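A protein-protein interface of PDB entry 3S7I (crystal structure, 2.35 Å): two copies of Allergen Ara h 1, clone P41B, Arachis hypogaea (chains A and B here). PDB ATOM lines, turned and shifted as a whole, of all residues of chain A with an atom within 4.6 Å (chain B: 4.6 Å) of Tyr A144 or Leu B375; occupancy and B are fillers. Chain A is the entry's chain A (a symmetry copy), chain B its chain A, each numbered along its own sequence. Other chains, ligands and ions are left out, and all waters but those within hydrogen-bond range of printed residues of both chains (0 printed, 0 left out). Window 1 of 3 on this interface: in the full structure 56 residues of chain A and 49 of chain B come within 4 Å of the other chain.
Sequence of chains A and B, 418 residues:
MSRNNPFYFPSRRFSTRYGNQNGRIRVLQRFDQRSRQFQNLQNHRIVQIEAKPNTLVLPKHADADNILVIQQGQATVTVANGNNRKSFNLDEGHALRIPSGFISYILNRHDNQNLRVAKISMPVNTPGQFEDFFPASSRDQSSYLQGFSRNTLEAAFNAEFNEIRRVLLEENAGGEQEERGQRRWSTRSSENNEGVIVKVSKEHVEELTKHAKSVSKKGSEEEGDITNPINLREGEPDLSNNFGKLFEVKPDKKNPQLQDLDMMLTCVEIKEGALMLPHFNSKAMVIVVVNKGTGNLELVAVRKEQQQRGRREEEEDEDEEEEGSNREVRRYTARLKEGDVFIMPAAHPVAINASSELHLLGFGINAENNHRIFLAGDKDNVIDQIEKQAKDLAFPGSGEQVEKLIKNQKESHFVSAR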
ATOM      1  N   HIS A  61      -1.064   5.135  21.172  1.00  0.00           N
ATOM      2  CA  HIS A  61      -0.423   5.664  19.970  1.00  0.00           C
ATOM      3  C   HIS A  61       0.158   4.546  19.176  1.00  0.00           C
ATOM      4  O   HIS A  61       0.370   3.465  19.675  1.00  0.00           O
ATOM      5  CB  HIS A  61       0.633   6.685  20.332  1.00  0.00           C
ATOM      6  CG  HIS A  61       1.918   6.126  20.862  1.00  0.00           C
ATOM      7  ND1 HIS A  61       2.248   6.170  22.189  1.00  0.00           N
ATOM      8  CD2 HIS A  61       2.998   5.624  20.232  1.00  0.00           C
ATOM      9  CE1 HIS A  61       3.455   5.669  22.367  1.00  0.00           C
ATOM     10  NE2 HIS A  61       3.955   5.366  21.185  1.00  0.00           N
ATOM     11  N   PHE A 133       0.688   1.326  21.103  1.00  0.00           N
ATOM     12  CA  PHE A 133       1.399   1.486  22.395  1.00  0.00           C
ATOM     13  C   PHE A 133       0.390   2.114  23.356  1.00  0.00           C
ATOM     14  O   PHE A 133      -0.022   3.294  23.149  1.00  0.00           O
ATOM     15  CB  PHE A 133       2.569   2.439  22.279  1.00  0.00           C
ATOM     16  CG  PHE A 133       3.720   1.867  21.510  1.00  0.00           C
ATOM     17  CD1 PHE A 133       3.602   1.620  20.155  1.00  0.00           C
ATOM     18  CD2 PHE A 133       4.899   1.527  22.149  1.00  0.00           C
ATOM     19  CE1 PHE A 133       4.679   1.055  19.456  1.00  0.00           C
ATOM     20  CE2 PHE A 133       5.935   0.964  21.478  1.00  0.00           C
ATOM     21  CZ  PHE A 133       5.866   0.745  20.120  1.00  0.00           C
ATOM     22  N   PHE A 134      -0.004   1.324  24.368  1.00  0.00           N
ATOM     23  CA  PHE A 134      -1.013   1.706  25.341  1.00  0.00           C
ATOM     24  C   PHE A 134      -0.292   2.031  26.613  1.00  0.00           C
ATOM     25  O   PHE A 134       0.505   1.220  27.076  1.00  0.00           O
ATOM     26  CB  PHE A 134      -1.936   0.533  25.687  1.00  0.00           C
ATOM     27  CG  PHE A 134      -2.873   0.137  24.578  1.00  0.00           C
ATOM     28  CD1 PHE A 134      -2.492  -0.819  23.646  1.00  0.00           C
ATOM     29  CD2 PHE A 134      -4.131   0.675  24.508  1.00  0.00           C
ATOM     30  CE1 PHE A 134      -3.327  -1.207  22.637  1.00  0.00           C
ATOM     31  CE2 PHE A 134      -5.000   0.281  23.517  1.00  0.00           C
ATOM     32  CZ  PHE A 134      -4.604  -0.660  22.557  1.00  0.00           C
ATOM     33  N   PRO A 135      -0.557   3.208  27.178  1.00  0.00           N
ATOM     34  CA  PRO A 135       0.118   3.545  28.413  1.00  0.00           C
ATOM     35  C   PRO A 135      -0.446   2.804  29.642  1.00  0.00           C
ATOM     36  O   PRO A 135       0.267   2.764  30.645  1.00  0.00           O
ATOM     37  CB  PRO A 135      -0.107   5.054  28.536  1.00  0.00           C
ATOM     38  CG  PRO A 135      -1.394   5.315  27.758  1.00  0.00           C
ATOM     39  CD  PRO A 135      -1.438   4.287  26.677  1.00  0.00           C
ATOM     40  N   SER A 142      -0.112  -5.204  27.986  1.00  0.00           N
ATOM     41  CA  SER A 142       0.557  -4.457  29.049  1.00  0.00           C
ATOM     42  C   SER A 142       0.833  -2.975  28.724  1.00  0.00           C
ATOM     43  O   SER A 142       0.969  -2.567  27.540  1.00  0.00           O
ATOM     44  CB  SER A 142       1.869  -5.168  29.392  1.00  0.00           C
ATOM     45  OG  SER A 142       1.654  -6.296  30.279  1.00  0.00           O
ATOM     46  N   SER A 143       0.887  -2.162  29.751  1.00  0.00           N
ATOM     47  CA  SER A 143       1.474  -0.824  29.666  1.00  0.00           C
ATOM     48  C   SER A 143       2.920  -0.885  29.235  1.00  0.00           C
ATOM     49  O   SER A 143       3.704  -1.677  29.761  1.00  0.00           O
ATOM     50  CB  SER A 143       1.470  -0.115  31.029  1.00  0.00           C
ATOM     51  OG  SER A 143       2.069   1.182  30.906  1.00  0.00           O
ATOM     52  N   TYR A 144       3.314  -0.047  28.303  1.00  0.00           N
ATOM     53  CA  TYR A 144       4.759   0.068  27.940  1.00  0.00           C
ATOM     54  C   TYR A 144       5.624   0.611  29.058  1.00  0.00           C
ATOM     55  O   TYR A 144       6.840   0.497  28.974  1.00  0.00           O
ATOM     56  CB  TYR A 144       4.985   0.894  26.695  1.00  0.00           C
ATOM     57  CG  TYR A 144       4.272   2.208  26.601  1.00  0.00           C
ATOM     58  CD1 TYR A 144       4.734   3.320  27.292  1.00  0.00           C
ATOM     59  CD2 TYR A 144       3.150   2.361  25.784  1.00  0.00           C
ATOM     60  CE1 TYR A 144       4.104   4.557  27.193  1.00  0.00           C
ATOM     61  CE2 TYR A 144       2.510   3.594  25.669  1.00  0.00           C
ATOM     62  CZ  TYR A 144       2.992   4.686  26.389  1.00  0.00           C
ATOM     63  OH  TYR A 144       2.360   5.918  26.293  1.00  0.00           O
ATOM     64  N   LEU A 145       5.018   1.169  30.104  1.00  0.00           N
ATOM     65  CA  LEU A 145       5.760   1.645  31.265  1.00  0.00           C
ATOM     66  C   LEU A 145       6.304   0.505  32.042  1.00  0.00           C
ATOM     67  O   LEU A 145       7.328   0.643  32.703  1.00  0.00           O
ATOM     68  CB  LEU A 145       4.914   2.517  32.162  1.00  0.00           C
ATOM     69  CG  LEU A 145       4.310   3.786  31.531  1.00  0.00           C
ATOM     70  CD1 LEU A 145       3.353   4.444  32.484  1.00  0.00           C
ATOM     71  CD2 LEU A 145       5.368   4.766  31.031  1.00  0.00           C
ATOM     72  N   GLN A 146       5.651  -0.646  31.944  1.00  0.00           N
ATOM     73  CA  GLN A 146       6.168  -1.871  32.566  1.00  0.00           C
ATOM     74  C   GLN A 146       7.535  -2.247  32.046  1.00  0.00           C
ATOM     75  O   GLN A 146       8.312  -2.818  32.740  1.00  0.00           O
ATOM     76  CB  GLN A 146       5.202  -3.048  32.418  1.00  0.00           C
ATOM     77  CG  GLN A 146       4.017  -3.042  33.406  1.00  0.00           C
ATOM     78  CD  GLN A 146       3.080  -4.271  33.266  1.00  0.00           C
ATOM     79  OE1 GLN A 146       2.895  -4.808  32.175  1.00  0.00           O
ATOM     80  NE2 GLN A 146       2.489  -4.704  34.381  1.00  0.00           N
ATOM     81  N   GLY A 147       7.865  -1.868  30.833  1.00  0.00           N
ATOM     82  CA  GLY A 147       9.178  -2.144  30.267  1.00  0.00           C
ATOM     83  C   GLY A 147      10.328  -1.355  30.843  1.00  0.00           C
ATOM     84  O   GLY A 147      11.460  -1.693  30.574  1.00  0.00           O
ATOM     85  N   PHE A 148      10.033  -0.283  31.582  1.00  0.00           N
ATOM     86  CA  PHE A 148      11.034   0.496  32.317  1.00  0.00           C
ATOM     87  C   PHE A 148      11.345  -0.132  33.670  1.00  0.00           C
ATOM     88  O   PHE A 148      10.528  -0.843  34.223  1.00  0.00           O
ATOM     89  CB  PHE A 148      10.583   1.957  32.435  1.00  0.00           C
ATOM     90  CG  PHE A 148      10.703   2.725  31.142  1.00  0.00           C
ATOM     91  CD1 PHE A 148       9.570   3.072  30.406  1.00  0.00           C
ATOM     92  CD2 PHE A 148      11.941   3.023  30.610  1.00  0.00           C
ATOM     93  CE1 PHE A 148       9.672   3.729  29.217  1.00  0.00           C
ATOM     94  CE2 PHE A 148      12.070   3.673  29.419  1.00  0.00           C
ATOM     95  CZ  PHE A 148      10.919   4.037  28.723  1.00  0.00           C
ATOM     96  N   PHE A 157       8.641   9.556  37.904  1.00  0.00           N
ATOM     97  CA  PHE A 157       7.447  10.082  38.497  1.00  0.00           C
ATOM     98  C   PHE A 157       7.638  10.649  39.880  1.00  0.00           C
ATOM     99  O   PHE A 157       6.734  11.271  40.385  1.00  0.00           O
ATOM    100  CB  PHE A 157       6.351   9.026  38.507  1.00  0.00           C
ATOM    101  CG  PHE A 157       5.977   8.520  37.146  1.00  0.00           C
ATOM    102  CD1 PHE A 157       5.106   9.206  36.351  1.00  0.00           C
ATOM    103  CD2 PHE A 157       6.481   7.350  36.688  1.00  0.00           C
ATOM    104  CE1 PHE A 157       4.770   8.727  35.142  1.00  0.00           C
ATOM    105  CE2 PHE A 157       6.146   6.886  35.493  1.00  0.00           C
ATOM    106  CZ  PHE A 157       5.285   7.567  34.722  1.00  0.00           C
ATOM    107  N   PRO B 278      11.624   9.076  30.272  1.00  0.00           N
ATOM    108  CA  PRO B 278      11.005   8.216  29.269  1.00  0.00           C
ATOM    109  C   PRO B 278      10.257   9.087  28.278  1.00  0.00           C
ATOM    110  O   PRO B 278       9.452   9.901  28.620  1.00  0.00           O
ATOM    111  CB  PRO B 278      10.028   7.419  30.107  1.00  0.00           C
ATOM    112  CG  PRO B 278      10.685   7.335  31.428  1.00  0.00           C
ATOM    113  CD  PRO B 278      11.488   8.540  31.624  1.00  0.00           C
ATOM    114  N   HIS B 279      10.558   8.868  27.024  1.00  0.00           N
ATOM    115  CA  HIS B 279      10.108   9.711  25.963  1.00  0.00           C
ATOM    116  C   HIS B 279      10.272   8.973  24.672  1.00  0.00           C
ATOM    117  O   HIS B 279      10.738   7.876  24.659  1.00  0.00           O
ATOM    118  CB  HIS B 279      10.973  10.959  25.940  1.00  0.00           C
ATOM    119  CG  HIS B 279      12.365  10.705  25.465  1.00  0.00           C
ATOM    120  ND1 HIS B 279      13.367  10.279  26.298  1.00  0.00           N
ATOM    121  CD2 HIS B 279      12.910  10.769  24.235  1.00  0.00           C
ATOM    122  CE1 HIS B 279      14.471  10.111  25.611  1.00  0.00           C
ATOM    123  NE2 HIS B 279      14.219  10.398  24.355  1.00  0.00           N
ATOM    124  N   PHE B 280       9.844   9.586  23.591  1.00  0.00           N
ATOM    125  CA  PHE B 280       9.993   8.997  22.258  1.00  0.00           C
ATOM    126  C   PHE B 280       9.821  10.094  21.317  1.00  0.00           C
ATOM    127  O   PHE B 280       9.307  11.158  21.678  1.00  0.00           O
ATOM    128  CB  PHE B 280       8.979   7.900  22.032  1.00  0.00           C
ATOM    129  CG  PHE B 280       7.530   8.357  22.129  1.00  0.00           C
ATOM    130  CD1 PHE B 280       6.944   9.071  21.100  1.00  0.00           C
ATOM    131  CD2 PHE B 280       6.734   7.955  23.158  1.00  0.00           C
ATOM    132  CE1 PHE B 280       5.624   9.444  21.144  1.00  0.00           C
ATOM    133  CE2 PHE B 280       5.406   8.340  23.202  1.00  0.00           C
ATOM    134  CZ  PHE B 280       4.864   9.095  22.187  1.00  0.00           C
ATOM    135  N   VAL B 300      11.820   0.462  25.070  1.00  0.00           N
ATOM    136  CA  VAL B 300      10.647  -0.413  25.111  1.00  0.00           C
ATOM    137  C   VAL B 300      10.001  -0.574  23.765  1.00  0.00           C
ATOM    138  O   VAL B 300       9.683   0.403  23.133  1.00  0.00           O
ATOM    139  CB  VAL B 300       9.621   0.072  26.161  1.00  0.00           C
ATOM    140  CG1 VAL B 300       8.534  -0.873  26.249  1.00  0.00           C
ATOM    141  CG2 VAL B 300      10.368   0.239  27.513  1.00  0.00           C
ATOM    142  N   VAL B 329       4.887  -6.390  25.629  1.00  0.00           N
ATOM    143  CA  VAL B 329       5.937  -5.409  25.898  1.00  0.00           C
ATOM    144  C   VAL B 329       7.257  -6.122  26.130  1.00  0.00           C
ATOM    145  O   VAL B 329       7.310  -7.065  26.884  1.00  0.00           O
ATOM    146  CB  VAL B 329       5.574  -4.503  27.062  1.00  0.00           C
ATOM    147  CG1 VAL B 329       6.783  -3.638  27.514  1.00  0.00           C
ATOM    148  CG2 VAL B 329       4.411  -3.611  26.640  1.00  0.00           C
ATOM    149  N   PRO B 349       9.295   4.072  23.360  1.00  0.00           N
ATOM    150  CA  PRO B 349       9.818   4.691  24.564  1.00  0.00           C
ATOM    151  C   PRO B 349      11.265   4.370  24.892  1.00  0.00           C
ATOM    152  O   PRO B 349      11.708   3.236  24.787  1.00  0.00           O
ATOM    153  CB  PRO B 349       8.898   4.147  25.657  1.00  0.00           C
ATOM    154  CG  PRO B 349       7.567   3.908  24.945  1.00  0.00           C
ATOM    155  CD  PRO B 349       7.957   3.501  23.580  1.00  0.00           C
ATOM    156  N   ILE B 373       8.256  13.465  22.579  1.00  0.00           N
ATOM    157  CA  ILE B 373       7.145  13.423  23.518  1.00  0.00           C
ATOM    158  C   ILE B 373       7.552  12.701  24.758  1.00  0.00           C
ATOM    159  O   ILE B 373       8.071  11.596  24.708  1.00  0.00           O
ATOM    160  CB  ILE B 373       5.953  12.730  22.871  1.00  0.00           C
ATOM    161  CG1 ILE B 373       5.484  13.554  21.682  1.00  0.00           C
ATOM    162  CG2 ILE B 373       4.796  12.565  23.826  1.00  0.00           C
ATOM    163  CD1 ILE B 373       4.123  13.135  21.130  1.00  0.00           C
ATOM    164  N   PHE B 374       7.263  13.295  25.912  1.00  0.00           N
ATOM    165  CA  PHE B 374       7.607  12.650  27.166  1.00  0.00           C
ATOM    166  C   PHE B 374       6.455  12.022  27.831  1.00  0.00           C
ATOM    167  O   PHE B 374       5.337  12.287  27.502  1.00  0.00           O
ATOM    168  CB  PHE B 374       8.278  13.619  28.110  1.00  0.00           C
ATOM    169  CG  PHE B 374       9.676  13.941  27.707  1.00  0.00           C
ATOM    170  CD1 PHE B 374      10.758  13.523  28.470  1.00  0.00           C
ATOM    171  CD2 PHE B 374       9.907  14.683  26.580  1.00  0.00           C
ATOM    172  CE1 PHE B 374      12.075  13.829  28.070  1.00  0.00           C
ATOM    173  CE2 PHE B 374      11.171  14.980  26.198  1.00  0.00           C
ATOM    174  CZ  PHE B 374      12.281  14.568  26.983  1.00  0.00           C
ATOM    175  N   LEU B 375       6.773  11.172  28.792  1.00  0.00           N
ATOM    176  CA  LEU B 375       5.843  10.351  29.448  1.00  0.00           C
ATOM    177  C   LEU B 375       5.803  10.628  30.966  1.00  0.00           C
ATOM    178  O   LEU B 375       5.018  10.012  31.717  1.00  0.00           O
ATOM    179  CB  LEU B 375       6.247   8.914  29.214  1.00  0.00           C
ATOM    180  CG  LEU B 375       6.146   8.505  27.780  1.00  0.00           C
ATOM    181  CD1 LEU B 375       6.933   7.264  27.609  1.00  0.00           C
ATOM    182  CD2 LEU B 375       4.637   8.320  27.381  1.00  0.00           C
ATOM    183  N   ALA B 376       6.632  11.561  31.394  1.00  0.00           N
ATOM    184  CA  ALA B 376       6.731  11.947  32.783  1.00  0.00           C
ATOM    185  C   ALA B 376       7.259  13.345  32.882  1.00  0.00           C
ATOM    186  O   ALA B 376       7.774  13.886  31.926  1.00  0.00           O
ATOM    187  CB  ALA B 376       7.601  11.006  33.540  1.00  0.00           C
ATOM    188  N   ASN B 381       4.575  16.230  28.436  1.00  0.00           N
ATOM    189  CA  ASN B 381       4.025  14.980  28.993  1.00  0.00           C
ATOM    190  C   ASN B 381       2.661  14.645  28.373  1.00  0.00           C
ATOM    191  O   ASN B 381       1.701  15.285  28.672  1.00  0.00           O
ATOM    192  CB  ASN B 381       3.861  15.121  30.503  1.00  0.00           C
ATOM    193  CG  ASN B 381       3.599  13.798  31.160  1.00  0.00           C
ATOM    194  OD1 ASN B 381       3.153  12.864  30.457  1.00  0.00           O
ATOM    195  ND2 ASN B 381       3.879  13.676  32.493  1.00  0.00           N
ATOM    196  N   VAL B 382       2.613  13.653  27.495  1.00  0.00           N
ATOM    197  CA  VAL B 382       1.406  13.350  26.708  1.00  0.00           C
ATOM    198  C   VAL B 382       0.338  12.699  27.571  1.00  0.00           C
ATOM    199  O   VAL B 382      -0.862  12.834  27.296  1.00  0.00           O
ATOM    200  CB  VAL B 382       1.754  12.479  25.452  1.00  0.00           C
ATOM    201  CG1 VAL B 382       2.423  11.208  25.860  1.00  0.00           C
ATOM    202  CG2 VAL B 382       0.549  12.228  24.548  1.00  0.00           C
ATOM    203  N   ILE B 383       0.757  12.049  28.646  1.00  0.00           N
ATOM    204  CA  ILE B 383      -0.166  11.396  29.563  1.00  0.00           C
ATOM    205  C   ILE B 383      -0.993  12.440  30.329  1.00  0.00           C
ATOM    206  O   ILE B 383      -2.221  12.362  30.365  1.00  0.00           O
ATOM    207  CB  ILE B 383       0.592  10.512  30.493  1.00  0.00           C
ATOM    208  CG1 ILE B 383       1.335   9.436  29.661  1.00  0.00           C
ATOM    209  CG2 ILE B 383      -0.322   9.951  31.514  1.00  0.00           C
ATOM    210  CD1 ILE B 383       2.032   8.380  30.502  1.00  0.00           C
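Of the 12 printed residues of chain A, 8 touch a printed residue of chain B.
Printed residues of chain B that touch a printed residue of chain A: Pro B278, Phe B280, Val B300, Val B329, Pro B349, Leu B375 and Ala B376.
Along chain B the printed residues that touch a printed residue of chain A span positions 278 to 376.
Among the printed residues, 15 pairs touch across the chains.
The backbone carbonyl oxygen (O) of His A61 sits at hydrogen-bond distance from the backbone NH (N) of Phe A133, at 2.6 Å.
The side-chain amide oxygen (OE1) of Gln A146 sits at hydrogen-bond distance from the side-chain hydroxyl (OG) of Ser A142 (2.7 Å).
The backbone carbonyl oxygen (O) of Pro B349 sits at hydrogen-bond distance from the backbone NH (N) of Val B300, at 2.8 Å.
The backbone NH (N) of Tyr A144 lies close to the backbone carbonyl oxygen (O) of Phe A134.
The backbone carbonyl oxygen (O) of Phe B280 is in hydrogen-bond range of the backbone NH (N) of Ile B373 (2.7 Å).
O of Pro A135 lies within hydrogen-bond range of OG of Ser A143 (2.4 Å).
No position is printed for both chains.
His A61 touches Phe B280.
Val B329 touches Ser A142 (CG2 to O, 3.7 Å).
Ser A143 touches Val B329.
Tyr A144 touches Val B300.
Tyr A144 touches Pro B349.
Gly A147 touches Val B329 (N to CG1, 3.9 Å).
Phe A148 touches Pro B278.
CE1 of Phe A148 touches CG2 of Val B300 (3.9 Å).
CE1 of Phe A148 touches CB of Pro B349 (3.7 Å).
Phe A157 touches Leu B375.
Of chain B, only Val B300 (3.5 Å), Val B329 (3.9 Å), Pro B349 (3.7 Å) and Leu B375 (3.5 Å) come within 4 Å of Tyr A144.
Printed residues of chain A within 4 Å of Ala B376: Phe A157.
Of the printed residues of chain B, Ser A143 touches Val B329.
Of the printed residues of chain B, Phe A133 touches Pro B349.
Ile B373 touches none of the printed residues of chain A.
The nearest printed residue of chain B that does not touch Tyr A144 is Ile B383 (4.9 Å).
The nearest printed residue of chain A that does not touch Phe B280 is Tyr A144 (5.0 Å).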
